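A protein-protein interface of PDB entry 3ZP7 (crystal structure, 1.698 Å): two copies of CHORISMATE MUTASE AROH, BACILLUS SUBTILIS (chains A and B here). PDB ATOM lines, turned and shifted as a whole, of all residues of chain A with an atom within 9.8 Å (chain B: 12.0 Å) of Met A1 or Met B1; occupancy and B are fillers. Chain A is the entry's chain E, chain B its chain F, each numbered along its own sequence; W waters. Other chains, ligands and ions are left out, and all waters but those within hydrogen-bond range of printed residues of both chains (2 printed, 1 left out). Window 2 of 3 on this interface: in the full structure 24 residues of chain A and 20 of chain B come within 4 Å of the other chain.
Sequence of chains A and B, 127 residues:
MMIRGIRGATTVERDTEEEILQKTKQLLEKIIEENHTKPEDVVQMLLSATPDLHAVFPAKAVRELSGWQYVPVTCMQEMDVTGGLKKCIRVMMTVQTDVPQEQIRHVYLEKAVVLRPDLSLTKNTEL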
ATOM      1  N   MET A   1      26.469 -17.069   0.589  1.00  0.00           N
ATOM      2  CA  MET A   1      27.702 -17.834   0.769  1.00  0.00           C
ATOM      3  C   MET A   1      28.696 -17.532  -0.348  1.00  0.00           C
ATOM      4  O   MET A   1      28.423 -17.784  -1.525  1.00  0.00           O
ATOM      5  CB  MET A   1      27.400 -19.334   0.817  1.00  0.00           C
ATOM      6  CG  MET A   1      28.570 -20.184   1.270  1.00  0.00           C
ATOM      7  SD  MET A   1      29.437 -19.409   2.640  1.00  0.00           S
ATOM      8  CE  MET A   1      30.039 -20.767   3.569  1.00  0.00           C
ATOM      9  N   MET A   2      29.851 -16.994   0.038  1.00  0.00           N
ATOM     10  CA  MET A   2      30.900 -16.623  -0.894  1.00  0.00           C
ATOM     11  C   MET A   2      31.559 -17.846  -1.528  1.00  0.00           C
ATOM     12  O   MET A   2      31.510 -18.944  -0.989  1.00  0.00           O
ATOM     13  CB  MET A   2      31.940 -15.759  -0.156  1.00  0.00           C
ATOM     14  CG  MET A   2      33.083 -15.234  -1.008  1.00  0.00           C
ATOM     15  SD  MET A   2      32.531 -14.299  -2.448  1.00  0.00           S
ATOM     16  CE  MET A   2      34.129 -13.764  -3.078  1.00  0.00           C
ATOM     17  N   ILE A   3      32.182 -17.626  -2.684  1.00  0.00           N
ATOM     18  CA  ILE A   3      32.963 -18.632  -3.390  1.00  0.00           C
ATOM     19  C   ILE A   3      34.436 -18.219  -3.357  1.00  0.00           C
ATOM     20  O   ILE A   3      34.736 -17.037  -3.393  1.00  0.00           O
ATOM     21  CB  ILE A   3      32.529 -18.662  -4.859  1.00  0.00           C
ATOM     22  CG1 ILE A   3      31.005 -18.696  -4.939  1.00  0.00           C
ATOM     23  CG2 ILE A   3      33.160 -19.827  -5.567  1.00  0.00           C
ATOM     24  CD1 ILE A   3      30.407 -19.947  -4.298  1.00  0.00           C
ATOM     25  N   ARG A   4      35.352 -19.185  -3.273  1.00  0.00           N
ATOM     26  CA  ARG A   4      36.782 -18.858  -3.216  1.00  0.00           C
ATOM     27  C   ARG A   4      37.593 -19.859  -4.012  1.00  0.00           C
ATOM     28  O   ARG A   4      37.318 -21.061  -3.972  1.00  0.00           O
ATOM     29  CB  ARG A   4      37.297 -18.906  -1.771  1.00  0.00           C
ATOM     30  CG  ARG A   4      36.608 -17.936  -0.813  1.00  0.00           C
ATOM     31  CD  ARG A   4      37.393 -16.658  -0.663  1.00  0.00           C
ATOM     32  NE  ARG A   4      36.651 -15.628   0.070  1.00  0.00           N
ATOM     33  CZ  ARG A   4      36.641 -14.348  -0.283  1.00  0.00           C
ATOM     34  NH1 ARG A   4      37.323 -13.965  -1.354  1.00  0.00           N
ATOM     35  NH2 ARG A   4      35.941 -13.457   0.423  1.00  0.00           N
ATOM     36  N   ASP A  41      30.538 -29.077  -2.304  1.00  0.00           N
ATOM     37  CA  ASP A  41      30.782 -27.642  -2.185  1.00  0.00           C
ATOM     38  C   ASP A  41      31.755 -27.128  -3.250  1.00  0.00           C
ATOM     39  O   ASP A  41      32.085 -25.941  -3.294  1.00  0.00           O
ATOM     40  CB  ASP A  41      31.319 -27.333  -0.789  1.00  0.00           C
ATOM     41  CG  ASP A  41      30.303 -27.633   0.291  1.00  0.00           C
ATOM     42  OD1 ASP A  41      29.126 -27.275   0.081  1.00  0.00           O
ATOM     43  OD2 ASP A  41      30.665 -28.235   1.324  1.00  0.00           O
ATOM     44  N   VAL A  43      32.548 -25.974  -6.844  1.00  0.00           N
ATOM     45  CA  VAL A  43      31.891 -25.461  -8.040  1.00  0.00           C
ATOM     46  C   VAL A  43      32.464 -26.177  -9.251  1.00  0.00           C
ATOM     47  O   VAL A  43      31.735 -26.713 -10.095  1.00  0.00           O
ATOM     48  CB  VAL A  43      32.190 -23.962  -8.180  1.00  0.00           C
ATOM     49  CG1 VAL A  43      31.690 -23.405  -9.500  1.00  0.00           C
ATOM     50  CG2 VAL A  43      31.590 -23.204  -6.990  1.00  0.00           C
ATOM     51  N   VAL A  95      35.530 -23.243  -4.581  1.00  0.00           N
ATOM     52  CA  VAL A  95      34.679 -23.846  -3.536  1.00  0.00           C
ATOM     53  C   VAL A  95      33.797 -22.810  -2.848  1.00  0.00           C
ATOM     54  O   VAL A  95      34.195 -21.656  -2.687  1.00  0.00           O
ATOM     55  CB  VAL A  95      35.513 -24.564  -2.430  1.00  0.00           C
ATOM     56  CG1 VAL A  95      36.589 -25.456  -3.036  1.00  0.00           C
ATOM     57  CG2 VAL A  95      36.151 -23.567  -1.492  1.00  0.00           C
ATOM     58  N   GLN A  96      32.599 -23.215  -2.435  1.00  0.00           N
ATOM     59  CA  GLN A  96      31.809 -22.332  -1.580  1.00  0.00           C
ATOM     60  C   GLN A  96      32.303 -22.468  -0.135  1.00  0.00           C
ATOM     61  O   GLN A  96      32.500 -23.581   0.364  1.00  0.00           O
ATOM     62  CB  GLN A  96      30.292 -22.557  -1.725  1.00  0.00           C
ATOM     63  CG  GLN A  96      29.723 -23.812  -1.117  1.00  0.00           C
ATOM     64  CD  GLN A  96      28.201 -23.738  -0.919  1.00  0.00           C
ATOM     65  OE1 GLN A  96      27.575 -22.688  -1.086  1.00  0.00           O
ATOM     66  NE2 GLN A  96      27.611 -24.864  -0.568  1.00  0.00           N
ATOM     67  N   THR A  97      32.548 -21.324   0.508  1.00  0.00           N
ATOM     68  CA  THR A  97      33.134 -21.270   1.841  1.00  0.00           C
ATOM     69  C   THR A  97      33.033 -19.862   2.428  1.00  0.00           C
ATOM     70  O   THR A  97      33.064 -18.871   1.690  1.00  0.00           O
ATOM     71  CB  THR A  97      34.623 -21.724   1.836  1.00  0.00           C
ATOM     72  OG1 THR A  97      35.143 -21.724   3.170  1.00  0.00           O
ATOM     73  CG2 THR A  97      35.488 -20.807   0.971  1.00  0.00           C
ATOM     74  N   ASP A  98      32.965 -19.820   3.763  1.00  0.00           N
ATOM     75  CA  ASP A  98      32.912 -18.608   4.570  1.00  0.00           C
ATOM     76  C   ASP A  98      34.298 -18.184   4.984  1.00  0.00           C
ATOM     77  O   ASP A  98      34.497 -17.069   5.462  1.00  0.00           O
ATOM     78  CB  ASP A  98      32.148 -18.876   5.867  1.00  0.00           C
ATOM     79  CG  ASP A  98      30.691 -18.538   5.764  1.00  0.00           C
ATOM     80  OD1 ASP A  98      30.340 -17.694   4.914  1.00  0.00           O
ATOM     81  OD2 ASP A  98      29.898 -19.121   6.533  1.00  0.00           O
ATOM     82  N   VAL A  99      35.241 -19.106   4.850  1.00  0.00           N
ATOM     83  CA  VAL A  99      36.599 -18.884   5.321  1.00  0.00           C
ATOM     84  C   VAL A  99      37.150 -17.647   4.629  1.00  0.00           C
ATOM     85  O   VAL A  99      37.061 -17.519   3.411  1.00  0.00           O
ATOM     86  CB  VAL A  99      37.501 -20.103   5.048  1.00  0.00           C
ATOM     87  CG1 VAL A  99      38.958 -19.765   5.299  1.00  0.00           C
ATOM     88  CG2 VAL A  99      37.058 -21.287   5.905  1.00  0.00           C
ATOM     89  N   PRO A 100      37.692 -16.709   5.416  1.00  0.00           N
ATOM     90  CA  PRO A 100      38.215 -15.461   4.863  1.00  0.00           C
ATOM     91  C   PRO A 100      39.330 -15.724   3.872  1.00  0.00           C
ATOM     92  O   PRO A 100      40.060 -16.709   4.002  1.00  0.00           O
ATOM     93  CB  PRO A 100      38.756 -14.745   6.101  1.00  0.00           C
ATOM     94  CG  PRO A 100      37.904 -15.258   7.197  1.00  0.00           C
ATOM     95  CD  PRO A 100      37.699 -16.692   6.891  1.00  0.00           C
ATOM     96  N   ILE A 104      42.415 -19.047   3.565  1.00  0.00           N
ATOM     97  CA  ILE A 104      42.344 -20.179   2.649  1.00  0.00           C
ATOM     98  C   ILE A 104      43.718 -20.852   2.601  1.00  0.00           C
ATOM     99  O   ILE A 104      44.750 -20.175   2.583  1.00  0.00           O
ATOM    100  CB  ILE A 104      41.908 -19.737   1.237  1.00  0.00           C
ATOM    101  CG1 ILE A 104      40.496 -19.134   1.267  1.00  0.00           C
ATOM    102  CG2 ILE A 104      41.939 -20.919   0.272  1.00  0.00           C
ATOM    103  CD1 ILE A 104      39.379 -20.148   1.549  1.00  0.00           C
ATOM    104  N   MET B   1      24.498 -18.287  -2.369  1.00  0.00           N
ATOM    105  CA  MET B   1      23.839 -18.579  -3.641  1.00  0.00           C
ATOM    106  C   MET B   1      24.751 -19.407  -4.535  1.00  0.00           C
ATOM    107  O   MET B   1      25.681 -18.871  -5.136  1.00  0.00           O
ATOM    108  CB  MET B   1      23.456 -17.288  -4.361  1.00  0.00           C
ATOM    109  CG  MET B   1      22.137 -17.383  -5.103  1.00  0.00           C
ATOM    110  SD  MET B   1      20.752 -17.593  -3.963  1.00  0.00           S
ATOM    111  CE  MET B   1      20.860 -16.075  -3.018  1.00  0.00           C
ATOM    112  N   MET B   2      24.462 -20.702  -4.644  1.00  0.00           N
ATOM    113  CA  MET B   2      25.419 -21.652  -5.205  1.00  0.00           C
ATOM    114  C   MET B   2      25.671 -21.533  -6.704  1.00  0.00           C
ATOM    115  O   MET B   2      24.797 -21.157  -7.500  1.00  0.00           O
ATOM    116  CB  MET B   2      25.071 -23.101  -4.838  1.00  0.00           C
ATOM    117  CG  MET B   2      26.216 -24.108  -5.046  1.00  0.00           C
ATOM    118  SD  MET B   2      27.862 -23.561  -4.461  1.00  0.00           S
ATOM    119  CE  MET B   2      28.868 -24.977  -4.906  1.00  0.00           C
ATOM    120  N   ILE B   3      26.898 -21.873  -7.056  1.00  0.00           N
ATOM    121  CA  ILE B   3      27.396 -21.787  -8.403  1.00  0.00           C
ATOM    122  C   ILE B   3      27.956 -23.157  -8.755  1.00  0.00           C
ATOM    123  O   ILE B   3      28.555 -23.814  -7.905  1.00  0.00           O
ATOM    124  CB  ILE B   3      28.520 -20.743  -8.461  1.00  0.00           C
ATOM    125  CG1 ILE B   3      28.032 -19.433  -7.854  1.00  0.00           C
ATOM    126  CG2 ILE B   3      28.929 -20.510  -9.862  1.00  0.00           C
ATOM    127  CD1 ILE B   3      26.951 -18.787  -8.673  1.00  0.00           C
ATOM    128  N   ARG B   4      27.746 -23.603  -9.993  1.00  0.00           N
ATOM    129  CA  ARG B   4      28.242 -24.917 -10.417  1.00  0.00           C
ATOM    130  C   ARG B   4      28.776 -24.894 -11.844  1.00  0.00           C
ATOM    131  O   ARG B   4      28.263 -24.175 -12.695  1.00  0.00           O
ATOM    132  CB  ARG B   4      27.144 -25.977 -10.298  1.00  0.00           C
ATOM    133  CG  ARG B   4      26.695 -26.186  -8.860  1.00  0.00           C
ATOM    134  CD  ARG B   4      26.353 -27.608  -8.501  1.00  0.00           C
ATOM    135  NE  ARG B   4      25.913 -27.665  -7.108  1.00  0.00           N
ATOM    136  CZ  ARG B   4      26.719 -27.891  -6.074  1.00  0.00           C
ATOM    137  NH1 ARG B   4      28.011 -28.112  -6.273  1.00  0.00           N
ATOM    138  NH2 ARG B   4      26.224 -27.916  -4.844  1.00  0.00           N
ATOM    139  N   GLY B   5      29.789 -25.709 -12.110  1.00  0.00           N
ATOM    140  CA  GLY B   5      30.298 -25.825 -13.469  1.00  0.00           C
ATOM    141  C   GLY B   5      29.508 -26.844 -14.266  1.00  0.00           C
ATOM    142  O   GLY B   5      29.149 -27.903 -13.743  1.00  0.00           O
ATOM    143  N   GLU B  40      21.750 -14.620 -18.173  1.00  0.00           N
ATOM    144  CA  GLU B  40      22.027 -13.773 -17.012  1.00  0.00           C
ATOM    145  C   GLU B  40      22.515 -14.564 -15.800  1.00  0.00           C
ATOM    146  O   GLU B  40      23.087 -13.984 -14.861  1.00  0.00           O
ATOM    147  CB  GLU B  40      20.788 -12.950 -16.639  1.00  0.00           C
ATOM    148  CG  GLU B  40      19.575 -13.794 -16.242  1.00  0.00           C
ATOM    149  CD  GLU B  40      18.591 -14.034 -17.393  1.00  0.00           C
ATOM    150  OE1 GLU B  40      19.018 -14.119 -18.569  1.00  0.00           O
ATOM    151  OE2 GLU B  40      17.379 -14.143 -17.108  1.00  0.00           O
ATOM    152  N   ASP B  41      22.299 -15.881 -15.809  1.00  0.00           N
ATOM    153  CA  ASP B  41      22.734 -16.708 -14.681  1.00  0.00           C
ATOM    154  C   ASP B  41      24.129 -17.302 -14.889  1.00  0.00           C
ATOM    155  O   ASP B  41      24.644 -18.000 -14.024  1.00  0.00           O
ATOM    156  CB  ASP B  41      21.724 -17.824 -14.393  1.00  0.00           C
ATOM    157  CG  ASP B  41      20.377 -17.292 -13.904  1.00  0.00           C
ATOM    158  OD1 ASP B  41      20.345 -16.223 -13.252  1.00  0.00           O
ATOM    159  OD2 ASP B  41      19.346 -17.950 -14.168  1.00  0.00           O
ATOM    160  N   VAL B  42      24.731 -17.031 -16.043  1.00  0.00           N
ATOM    161  CA  VAL B  42      26.072 -17.541 -16.330  1.00  0.00           C
ATOM    162  C   VAL B  42      27.118 -16.571 -15.800  1.00  0.00           C
ATOM    163  O   VAL B  42      27.162 -15.412 -16.212  1.00  0.00           O
ATOM    164  CB  VAL B  42      26.272 -17.774 -17.841  1.00  0.00           C
ATOM    165  CG1 VAL B  42      27.672 -18.332 -18.125  1.00  0.00           C
ATOM    166  CG2 VAL B  42      25.210 -18.732 -18.363  1.00  0.00           C
ATOM    167  N   VAL B  43      27.914 -17.040 -14.841  1.00  0.00           N
ATOM    168  CA  VAL B  43      29.007 -16.264 -14.279  1.00  0.00           C
ATOM    169  C   VAL B  43      30.040 -15.954 -15.360  1.00  0.00           C
ATOM    170  O   VAL B  43      30.437 -14.792 -15.555  1.00  0.00           O
ATOM    171  CB  VAL B  43      29.706 -17.084 -13.176  1.00  0.00           C
ATOM    172  CG1 VAL B  43      30.861 -16.318 -12.573  1.00  0.00           C
ATOM    173  CG2 VAL B  43      28.712 -17.505 -12.105  1.00  0.00           C
ATOM    174  N   THR B  94      30.129 -21.858 -16.117  1.00  0.00           N
ATOM    175  CA  THR B  94      29.904 -21.680 -14.683  1.00  0.00           C
ATOM    176  C   THR B  94      28.605 -20.924 -14.475  1.00  0.00           C
ATOM    177  O   THR B  94      28.455 -19.816 -14.963  1.00  0.00           O
ATOM    178  CB  THR B  94      31.064 -20.860 -14.076  1.00  0.00           C
ATOM    179  OG1 THR B  94      32.304 -21.468 -14.453  1.00  0.00           O
ATOM    180  CG2 THR B  94      30.985 -20.815 -12.559  1.00  0.00           C
ATOM    181  N   VAL B  95      27.663 -21.529 -13.755  1.00  0.00           N
ATOM    182  CA  VAL B  95      26.310 -20.956 -13.659  1.00  0.00           C
ATOM    183  C   VAL B  95      25.785 -20.845 -12.232  1.00  0.00           C
ATOM    184  O   VAL B  95      26.179 -21.602 -11.354  1.00  0.00           O
ATOM    185  CB  VAL B  95      25.264 -21.752 -14.513  1.00  0.00           C
ATOM    186  CG1 VAL B  95      25.732 -21.924 -15.977  1.00  0.00           C
ATOM    187  CG2 VAL B  95      24.926 -23.113 -13.877  1.00  0.00           C
ATOM    188  N   GLN B  96      24.889 -19.882 -11.995  1.00  0.00           N
ATOM    189  CA  GLN B  96      24.125 -19.878 -10.758  1.00  0.00           C
ATOM    190  C   GLN B  96      22.959 -20.852 -10.916  1.00  0.00           C
ATOM    191  O   GLN B  96      22.138 -20.708 -11.821  1.00  0.00           O
ATOM    192  CB  GLN B  96      23.615 -18.466 -10.435  1.00  0.00           C
ATOM    193  CG  GLN B  96      22.938 -18.337  -9.064  1.00  0.00           C
ATOM    194  CD  GLN B  96      21.424 -18.490  -9.124  1.00  0.00           C
ATOM    195  OE1 GLN B  96      20.747 -17.794  -9.886  1.00  0.00           O
ATOM    196  NE2 GLN B  96      20.886 -19.401  -8.317  1.00  0.00           N
ATOM    197  N   THR B  97      22.899 -21.859 -10.051  1.00  0.00           N
ATOM    198  CA  THR B  97      21.846 -22.857 -10.131  1.00  0.00           C
ATOM    199  C   THR B  97      21.641 -23.525  -8.786  1.00  0.00           C
ATOM    200  O   THR B  97      22.561 -23.595  -7.967  1.00  0.00           O
ATOM    201  CB  THR B  97      22.163 -23.946 -11.172  1.00  0.00           C
ATOM    202  OG1 THR B  97      21.116 -24.928 -11.171  1.00  0.00           O
ATOM    203  CG2 THR B  97      23.494 -24.616 -10.858  1.00  0.00           C
ATOM    204  N   ASP B  98      20.423 -24.002  -8.558  1.00  0.00           N
ATOM    205  CA  ASP B  98      20.111 -24.747  -7.348  1.00  0.00           C
ATOM    206  C   ASP B  98      20.019 -26.242  -7.632  1.00  0.00           C
ATOM    207  O   ASP B  98      19.737 -27.034  -6.733  1.00  0.00           O
ATOM    208  CB  ASP B  98      18.818 -24.230  -6.715  1.00  0.00           C
ATOM    209  CG  ASP B  98      18.939 -22.791  -6.248  1.00  0.00           C
ATOM    210  OD1 ASP B  98      19.625 -22.556  -5.229  1.00  0.00           O
ATOM    211  OD2 ASP B  98      18.352 -21.900  -6.901  1.00  0.00           O
ATOM    212  N   VAL B  99      20.257 -26.626  -8.885  1.00  0.00           N
ATOM    213  CA  VAL B  99      20.305 -28.036  -9.251  1.00  0.00           C
ATOM    214  C   VAL B  99      21.489 -28.711  -8.558  1.00  0.00           C
ATOM    215  O   VAL B  99      22.621 -28.224  -8.643  1.00  0.00           O
ATOM    216  CB  VAL B  99      20.437 -28.223 -10.784  1.00  0.00           C
ATOM    217  CG1 VAL B  99      20.573 -29.700 -11.129  1.00  0.00           C
ATOM    218  CG2 VAL B  99      19.234 -27.614 -11.510  1.00  0.00           C
ATOM    219  N   PRO B 100      21.234 -29.833  -7.865  1.00  0.00           N
ATOM    220  CA  PRO B 100      22.297 -30.544  -7.150  1.00  0.00           C
ATOM    221  C   PRO B 100      23.392 -31.019  -8.095  1.00  0.00           C
ATOM    222  O   PRO B 100      23.131 -31.253  -9.278  1.00  0.00           O
ATOM    223  CB  PRO B 100      21.565 -31.742  -6.525  1.00  0.00           C
ATOM    224  CG  PRO B 100      20.320 -31.891  -7.326  1.00  0.00           C
ATOM    225  CD  PRO B 100      19.929 -30.495  -7.704  1.00  0.00           C
ATOM    226  N   ILE B 104      23.286 -32.103 -12.461  1.00  0.00           N
ATOM    227  CA  ILE B 104      23.767 -31.243 -13.536  1.00  0.00           C
ATOM    228  C   ILE B 104      23.970 -32.109 -14.778  1.00  0.00           C
ATOM    229  O   ILE B 104      24.542 -33.197 -14.693  1.00  0.00           O
ATOM    230  CB  ILE B 104      25.094 -30.543 -13.168  1.00  0.00           C
ATOM    231  CG1 ILE B 104      24.894 -29.566 -12.013  1.00  0.00           C
ATOM    232  CG2 ILE B 104      25.658 -29.776 -14.362  1.00  0.00           C
ATOM    233  CD1 ILE B 104      23.906 -28.460 -12.318  1.00  0.00           C
HETATM  234  O   HOH W   1      29.587 -28.646  -8.838  1.00  0.00           O
HETATM  235  O   HOH W   2      27.833 -17.369  -4.195  1.00  0.00           O
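N of Gly B5 lies within hydrogen-bond range of O of Val A43, 3.0 Å away. The side-chain amide oxygen (OE1) of Gln A96 sits close to the side-chain sulfur (SD) of Met B2, 3.5 Å away.
N of Asp A98 lies close to SD of Met A1, 3.7 Å away. The backbone NH (N) of Gln A96 lies within hydrogen-bond range of the backbone carbonyl oxygen (O) of Asp A41, 2.9 Å away. The backbone carbonyl oxygen (O) of Met B2 lies within hydrogen-bond range of the backbone NH (N) of Thr B97. O of Val B95 is in hydrogen-bond range of N of Arg B4, at 2.9 Å.
Met A1 touches its own counterpart, Met B1. Asp A41 touches Met B2, but with the chains exchanged Met A2 does not touch Asp B41 (14.3 Å). Val A43 touches Ile B3, but with the chains exchanged Ile A3 does not touch Val B43 (7.6 Å). Gln A96 touches Met B2, but with the chains exchanged Met A2 does not touch Gln B96 (11.5 Å). Positions printed for both chains: 1, 2, 3, 4, 41, 43, 95, 96, 97, 98, 99, 100 and 104.
Water W2 lies within hydrogen-bond range of the backbone carbonyl oxygen (O) of Met A1 (2.8 Å) and the backbone carbonyl oxygen (O) of Met B1 (2.8 Å). Water W1 bridges NH1 of Arg B4 (3.1 Å) and O of Val A43 (3.2 Å).
Of the printed residues of chain B, Met A1 touches Met B1. No residue of chain B comes within 4 Å of Met A2. Printed residues of chain B within 4 Å of Val A43: Met B2 (3.9 Å), Ile B3 (3.2 Å), Arg B4 (3.9 Å) and Gly B5 (3.0 Å). No residue of chain B comes within 4 Å of Thr A97. Printed residues of chain A within 4 Å of Met B1: Met A1. Of the printed residues of chain A, Met B2 touches Asp A41, Val A43 and Gln A96. Printed residues of chain A within 4 Å of Arg B4: Val A43 (3.9 Å). The nearest printed residue of chain A that does not touch Met B2 is Ile A3 (4.4 Å).
N of Met A1 touches N of Met B1, 3.8 Å away. CE of Met B2 touches O of Asp A41 (3.7 Å). Val A43 touches Met B2 (CG2 to CE, 3.9 Å). Val A43 touches Ile B3 (CG2 to O, 3.2 Å). Val A43 touches Arg B4 (CG1 to CA, 3.9 Å).
Printed residues of chain A that touch a printed residue of chain B: Met A1, Asp A41, Val A43 and Gln A96. Of the 17 printed residues of chain B, 5 touch a printed residue of chain A. Printed residues of chain B that touch a printed residue of chain A: Met B1, Met B2, Ile B3, Arg B4 and Gly B5.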
